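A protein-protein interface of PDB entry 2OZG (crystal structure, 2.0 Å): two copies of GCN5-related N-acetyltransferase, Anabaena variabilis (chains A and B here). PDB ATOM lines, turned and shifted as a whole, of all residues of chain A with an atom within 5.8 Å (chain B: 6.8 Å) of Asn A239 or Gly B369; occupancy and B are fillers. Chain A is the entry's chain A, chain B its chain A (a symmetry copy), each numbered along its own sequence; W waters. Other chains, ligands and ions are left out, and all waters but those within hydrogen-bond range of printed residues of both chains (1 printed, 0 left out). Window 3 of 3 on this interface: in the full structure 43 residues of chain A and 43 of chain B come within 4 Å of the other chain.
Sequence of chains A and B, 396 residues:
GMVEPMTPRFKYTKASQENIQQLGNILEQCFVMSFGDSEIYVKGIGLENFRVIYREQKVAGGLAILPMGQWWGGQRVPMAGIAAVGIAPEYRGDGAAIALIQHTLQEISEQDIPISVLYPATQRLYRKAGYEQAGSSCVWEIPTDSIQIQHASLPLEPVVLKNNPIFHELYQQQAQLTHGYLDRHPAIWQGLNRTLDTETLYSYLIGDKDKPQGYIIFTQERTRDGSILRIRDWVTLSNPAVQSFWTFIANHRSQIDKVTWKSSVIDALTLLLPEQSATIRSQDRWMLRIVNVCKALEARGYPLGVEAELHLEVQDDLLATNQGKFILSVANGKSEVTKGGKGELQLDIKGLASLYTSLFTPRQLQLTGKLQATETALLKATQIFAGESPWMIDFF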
ATOM      1  N   SER A 153      30.008  -5.431   7.987  1.00  0.00           N
ATOM      2  CA  SER A 153      29.173  -6.331   8.740  1.00  0.00           C
ATOM      3  C   SER A 153      29.932  -7.599   9.161  1.00  0.00           C
ATOM      4  O   SER A 153      29.790  -8.079  10.272  1.00  0.00           O
ATOM      5  CB  SER A 153      28.022  -6.768   7.816  1.00  0.00           C
ATOM      6  OG  SER A 153      27.394  -5.667   7.198  1.00  0.00           O
ATOM      7  N   LEU A 237      26.722 -14.629  -0.664  1.00  0.00           N
ATOM      8  CA  LEU A 237      25.471 -15.379  -0.468  1.00  0.00           C
ATOM      9  C   LEU A 237      24.385 -14.583   0.240  1.00  0.00           C
ATOM     10  O   LEU A 237      23.218 -14.962   0.186  1.00  0.00           O
ATOM     11  CB  LEU A 237      25.694 -16.689   0.266  1.00  0.00           C
ATOM     12  CG  LEU A 237      26.651 -17.679  -0.386  1.00  0.00           C
ATOM     13  CD1 LEU A 237      26.789 -18.920   0.491  1.00  0.00           C
ATOM     14  CD2 LEU A 237      26.170 -18.053  -1.779  1.00  0.00           C
ATOM     15  N   SER A 238      24.757 -13.454   0.835  1.00  0.00           N
ATOM     16  CA  SER A 238      23.844 -12.672   1.638  1.00  0.00           C
ATOM     17  C   SER A 238      24.230 -11.210   1.534  1.00  0.00           C
ATOM     18  O   SER A 238      25.332 -10.890   1.106  1.00  0.00           O
ATOM     19  CB  SER A 238      23.975 -13.109   3.098  1.00  0.00           C
ATOM     20  OG  SER A 238      25.260 -12.749   3.591  1.00  0.00           O
ATOM     21  N   ASN A 239      23.333 -10.341   1.965  1.00  0.00           N
ATOM     22  CA  ASN A 239      23.605  -8.909   1.950  1.00  0.00           C
ATOM     23  C   ASN A 239      24.784  -8.475   2.834  1.00  0.00           C
ATOM     24  O   ASN A 239      25.548  -7.599   2.445  1.00  0.00           O
ATOM     25  CB  ASN A 239      22.349  -8.131   2.319  1.00  0.00           C
ATOM     26  CG  ASN A 239      22.558  -6.644   2.189  1.00  0.00           C
ATOM     27  OD1 ASN A 239      23.106  -6.118   1.177  1.00  0.00           O
ATOM     28  ND2 ASN A 239      22.159  -5.963   3.213  1.00  0.00           N
ATOM     29  N   PRO A 240      24.903  -9.040   4.058  1.00  0.00           N
ATOM     30  CA  PRO A 240      26.110  -8.739   4.851  1.00  0.00           C
ATOM     31  C   PRO A 240      27.416  -9.100   4.089  1.00  0.00           C
ATOM     32  O   PRO A 240      28.413  -8.432   4.255  1.00  0.00           O
ATOM     33  CB  PRO A 240      25.927  -9.600   6.068  1.00  0.00           C
ATOM     34  CG  PRO A 240      24.430  -9.711   6.202  1.00  0.00           C
ATOM     35  CD  PRO A 240      23.954  -9.852   4.823  1.00  0.00           C
ATOM     36  N   ALA A 241      27.392 -10.147   3.262  1.00  0.00           N
ATOM     37  CA  ALA A 241      28.583 -10.488   2.465  1.00  0.00           C
ATOM     38  C   ALA A 241      28.786  -9.439   1.397  1.00  0.00           C
ATOM     39  O   ALA A 241      29.916  -9.067   1.141  1.00  0.00           O
ATOM     40  CB  ALA A 241      28.489 -11.875   1.861  1.00  0.00           C
ATOM     41  N   VAL A 242      27.696  -8.946   0.797  1.00  0.00           N
ATOM     42  CA  VAL A 242      27.802  -7.900  -0.223  1.00  0.00           C
ATOM     43  C   VAL A 242      28.360  -6.604   0.355  1.00  0.00           C
ATOM     44  O   VAL A 242      29.293  -6.051  -0.212  1.00  0.00           O
ATOM     45  CB  VAL A 242      26.495  -7.613  -1.017  1.00  0.00           C
ATOM     46  CG1 VAL A 242      26.753  -6.537  -2.072  1.00  0.00           C
ATOM     47  CG2 VAL A 242      25.958  -8.860  -1.703  1.00  0.00           C
ATOM     48  N   GLN A 243      27.837  -6.143   1.491  1.00  0.00           N
ATOM     49  CA  GLN A 243      28.357  -4.909   2.135  1.00  0.00           C
ATOM     50  C   GLN A 243      29.830  -5.039   2.505  1.00  0.00           C
ATOM     51  O   GLN A 243      30.633  -4.094   2.384  1.00  0.00           O
ATOM     52  CB  GLN A 243      27.570  -4.568   3.394  1.00  0.00           C
ATOM     53  CG  GLN A 243      26.111  -4.222   3.170  1.00  0.00           C
ATOM     54  CD  GLN A 243      25.842  -2.965   2.265  1.00  0.00           C
ATOM     55  OE1 GLN A 243      26.735  -2.153   2.009  1.00  0.00           O
ATOM     56  NE2 GLN A 243      24.577  -2.809   1.817  1.00  0.00           N
ATOM     57  N   SER A 244      30.177  -6.226   2.957  1.00  0.00           N
ATOM     58  CA  SER A 244      31.534  -6.552   3.383  1.00  0.00           C
ATOM     59  C   SER A 244      32.498  -6.577   2.202  1.00  0.00           C
ATOM     60  O   SER A 244      33.609  -6.099   2.272  1.00  0.00           O
ATOM     61  CB  SER A 244      31.500  -7.858   4.183  1.00  0.00           C
ATOM     62  OG  SER A 244      30.818  -7.683   5.456  1.00  0.00           O
ATOM     63  N   LEU A 272      24.088  -1.382  -4.745  1.00  0.00           N
ATOM     64  CA  LEU A 272      24.473  -0.860  -3.464  1.00  0.00           C
ATOM     65  C   LEU A 272      25.423   0.347  -3.451  1.00  0.00           C
ATOM     66  O   LEU A 272      25.659   0.902  -2.409  1.00  0.00           O
ATOM     67  CB  LEU A 272      25.049  -1.986  -2.617  1.00  0.00           C
ATOM     68  CG  LEU A 272      24.098  -3.160  -2.340  1.00  0.00           C
ATOM     69  CD1 LEU A 272      24.743  -4.075  -1.342  1.00  0.00           C
ATOM     70  CD2 LEU A 272      22.767  -2.665  -1.793  1.00  0.00           C
ATOM     71  N   GLN B 364      17.356 -11.413  -6.091  1.00  0.00           N
ATOM     72  CA  GLN B 364      18.414 -10.390  -6.203  1.00  0.00           C
ATOM     73  C   GLN B 364      18.195  -9.218  -5.238  1.00  0.00           C
ATOM     74  O   GLN B 364      19.129  -8.673  -4.713  1.00  0.00           O
ATOM     75  CB  GLN B 364      18.494  -9.851  -7.638  1.00  0.00           C
ATOM     76  CG  GLN B 364      19.185 -10.861  -8.606  1.00  0.00           C
ATOM     77  CD  GLN B 364      19.117 -10.413 -10.016  1.00  0.00           C
ATOM     78  OE1 GLN B 364      18.050  -9.954 -10.509  1.00  0.00           O
ATOM     79  NE2 GLN B 364      20.256 -10.517 -10.712  1.00  0.00           N
ATOM     80  N   LEU B 365      16.956  -8.812  -5.045  1.00  0.00           N
ATOM     81  CA  LEU B 365      16.643  -7.752  -4.091  1.00  0.00           C
ATOM     82  C   LEU B 365      16.828  -8.223  -2.612  1.00  0.00           C
ATOM     83  O   LEU B 365      17.292  -7.480  -1.730  1.00  0.00           O
ATOM     84  CB  LEU B 365      15.244  -7.229  -4.372  1.00  0.00           C
ATOM     85  CG  LEU B 365      15.093  -6.502  -5.718  1.00  0.00           C
ATOM     86  CD1 LEU B 365      13.629  -6.229  -6.104  1.00  0.00           C
ATOM     87  CD2 LEU B 365      15.927  -5.163  -5.734  1.00  0.00           C
ATOM     88  N   GLN B 366      16.541  -9.485  -2.360  1.00  0.00           N
ATOM     89  CA  GLN B 366      16.780 -10.050  -1.075  1.00  0.00           C
ATOM     90  C   GLN B 366      18.265 -10.033  -0.767  1.00  0.00           C
ATOM     91  O   GLN B 366      18.690  -9.625   0.313  1.00  0.00           O
ATOM     92  CB  GLN B 366      16.297 -11.484  -1.029  1.00  0.00           C
ATOM     93  CG  GLN B 366      16.438 -12.103   0.334  1.00  0.00           C
ATOM     94  CD  GLN B 366      16.047 -13.570   0.347  1.00  0.00           C
ATOM     95  OE1 GLN B 366      16.398 -14.350  -0.564  1.00  0.00           O
ATOM     96  NE2 GLN B 366      15.318 -13.950   1.364  1.00  0.00           N
ATOM     97  N   LEU B 367      19.048 -10.491  -1.726  1.00  0.00           N
ATOM     98  CA  LEU B 367      20.497 -10.599  -1.568  1.00  0.00           C
ATOM     99  C   LEU B 367      21.203  -9.268  -1.342  1.00  0.00           C
ATOM    100  O   LEU B 367      22.245  -9.239  -0.722  1.00  0.00           O
ATOM    101  CB  LEU B 367      21.080 -11.267  -2.803  1.00  0.00           C
ATOM    102  CG  LEU B 367      22.603 -11.345  -2.898  1.00  0.00           C
ATOM    103  CD1 LEU B 367      23.142 -12.257  -1.828  1.00  0.00           C
ATOM    104  CD2 LEU B 367      23.001 -11.834  -4.277  1.00  0.00           C
ATOM    105  N   THR B 368      20.647  -8.187  -1.896  1.00  0.00           N
ATOM    106  CA  THR B 368      21.190  -6.829  -1.800  1.00  0.00           C
ATOM    107  C   THR B 368      20.448  -6.033  -0.723  1.00  0.00           C
ATOM    108  O   THR B 368      20.586  -4.805  -0.614  1.00  0.00           O
ATOM    109  CB  THR B 368      21.136  -6.114  -3.163  1.00  0.00           C
ATOM    110  OG1 THR B 368      19.790  -6.056  -3.648  1.00  0.00           O
ATOM    111  CG2 THR B 368      21.985  -6.854  -4.195  1.00  0.00           C
ATOM    112  N   GLY B 369      19.643  -6.757   0.066  1.00  0.00           N
ATOM    113  CA  GLY B 369      18.991  -6.220   1.231  1.00  0.00           C
ATOM    114  C   GLY B 369      17.864  -5.238   1.022  1.00  0.00           C
ATOM    115  O   GLY B 369      17.552  -4.496   1.937  1.00  0.00           O
ATOM    116  N   LYS B 370      17.230  -5.253  -0.151  1.00  0.00           N
ATOM    117  CA  LYS B 370      16.147  -4.303  -0.424  1.00  0.00           C
ATOM    118  C   LYS B 370      14.775  -4.871  -0.067  1.00  0.00           C
ATOM    119  O   LYS B 370      13.748  -4.158  -0.128  1.00  0.00           O
ATOM    120  CB  LYS B 370      16.152  -3.923  -1.882  1.00  0.00           C
ATOM    121  CG  LYS B 370      17.514  -3.494  -2.316  1.00  0.00           C
ATOM    122  CD  LYS B 370      18.128  -2.460  -1.386  1.00  0.00           C
ATOM    123  CE  LYS B 370      19.271  -1.713  -2.109  1.00  0.00           C
ATOM    124  NZ  LYS B 370      19.965  -0.837  -1.119  1.00  0.00           N
ATOM    125  N   LEU B 371      14.742  -6.151   0.291  1.00  0.00           N
ATOM    126  CA  LEU B 371      13.504  -6.742   0.740  1.00  0.00           C
ATOM    127  C   LEU B 371      13.795  -7.948   1.638  1.00  0.00           C
ATOM    128  O   LEU B 371      14.879  -8.503   1.586  1.00  0.00           O
ATOM    129  CB  LEU B 371      12.580  -7.108  -0.432  1.00  0.00           C
ATOM    130  CG  LEU B 371      12.895  -8.162  -1.500  1.00  0.00           C
ATOM    131  CD1 LEU B 371      12.677  -9.577  -0.940  1.00  0.00           C
ATOM    132  CD2 LEU B 371      12.029  -7.998  -2.708  1.00  0.00           C
ATOM    133  N   GLN B 372      12.848  -8.251   2.523  1.00  0.00           N
ATOM    134  CA  GLN B 372      12.876  -9.461   3.335  1.00  0.00           C
ATOM    135  C   GLN B 372      11.578 -10.210   3.035  1.00  0.00           C
ATOM    136  O   GLN B 372      10.483  -9.606   2.992  1.00  0.00           O
ATOM    137  CB  GLN B 372      12.897  -9.118   4.830  1.00  0.00           C
ATOM    138  CG  GLN B 372      14.030  -8.213   5.213  1.00  0.00           C
ATOM    139  CD  GLN B 372      14.352  -8.313   6.712  1.00  0.00           C
ATOM    140  OE1 GLN B 372      13.480  -8.657   7.535  1.00  0.00           O
ATOM    141  NE2 GLN B 372      15.623  -8.033   7.062  1.00  0.00           N
HETATM  142  O   HOH W   1      20.716 -11.332   2.427  1.00  0.00           O
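The side-chain amide oxygen (OD1) of Asn A239 sits close to the backbone carbonyl oxygen (O) of Thr B368. N of Asn A239 lies close to O of Leu B367, at 3.1 Å.
The backbone NH (N) of Ala A241 lies within hydrogen-bond range of the side-chain hydroxyl (OG) of Ser A238, at 3.4 Å. OG1 of Thr B368 is in hydrogen-bond range of O of Gln B364 (2.9 Å). The backbone carbonyl oxygen (O) of Leu B365 lies within hydrogen-bond range of the backbone NH (N) of Lys B370 (2.7 Å). O of Leu B365 is in hydrogen-bond range of OG1 of Thr B368, at 3.5 Å.
Among the printed residues, merely in contact across the chains: Leu A272 with Thr B368 (3.3 Å), Ser A238 with Leu B367 (3.3 Å), Leu A237 with Leu B367 (3.4 Å), Leu A272 with Lys B370 (3.4 Å), Asn A239 with Gly B369 (3.6 Å) and Val A242 with Leu B367 (3.9 Å).
Printed residues of chain B within 4 Å of Ser A238: Leu B367 (3.3 Å). Asn A239 touches three residues of chain B. Leu B365 touches none of the printed residues of chain A. Printed residues of chain A within 4 Å of Thr B368: Asn A239 (3.3 Å) and Leu A272 (3.3 Å). Of the printed residues of chain A, Gly B369 touches Asn A239 (3.6 Å). The nearest residue of chain B that does not touch Asn A239 is Gln B366 (4.4 Å). The nearest printed residue of chain A that does not touch Thr B368 is Gln A243 (5.1 Å).
Of the 10 printed residues of chain A, 5 touch a printed residue of chain B. Hydrophobic or aromatic side chains of chain A within 4 Å of the printed part of chain B: Val A242 and Leu A272. Of the 9 printed residues of chain B, 4 touch a printed residue of chain A. Hydrophobic or aromatic side chains of chain B that line the printed part of chain A: Leu B367. Among the printed residues, 8 pairs touch across the chains. Among the printed residues, no Asp or Glu carboxylate lies within 4 Å of a Lys or Arg side-chain nitrogen of the other chain.
No position is printed for both chains. Of the 8 pairs that touch across the chains among the printed residues, none has its exchanged pair printed and touching as well.
Water W1 bridges N of Asn A239 (2.8 Å) and O of Gln B366 (3.4 Å).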
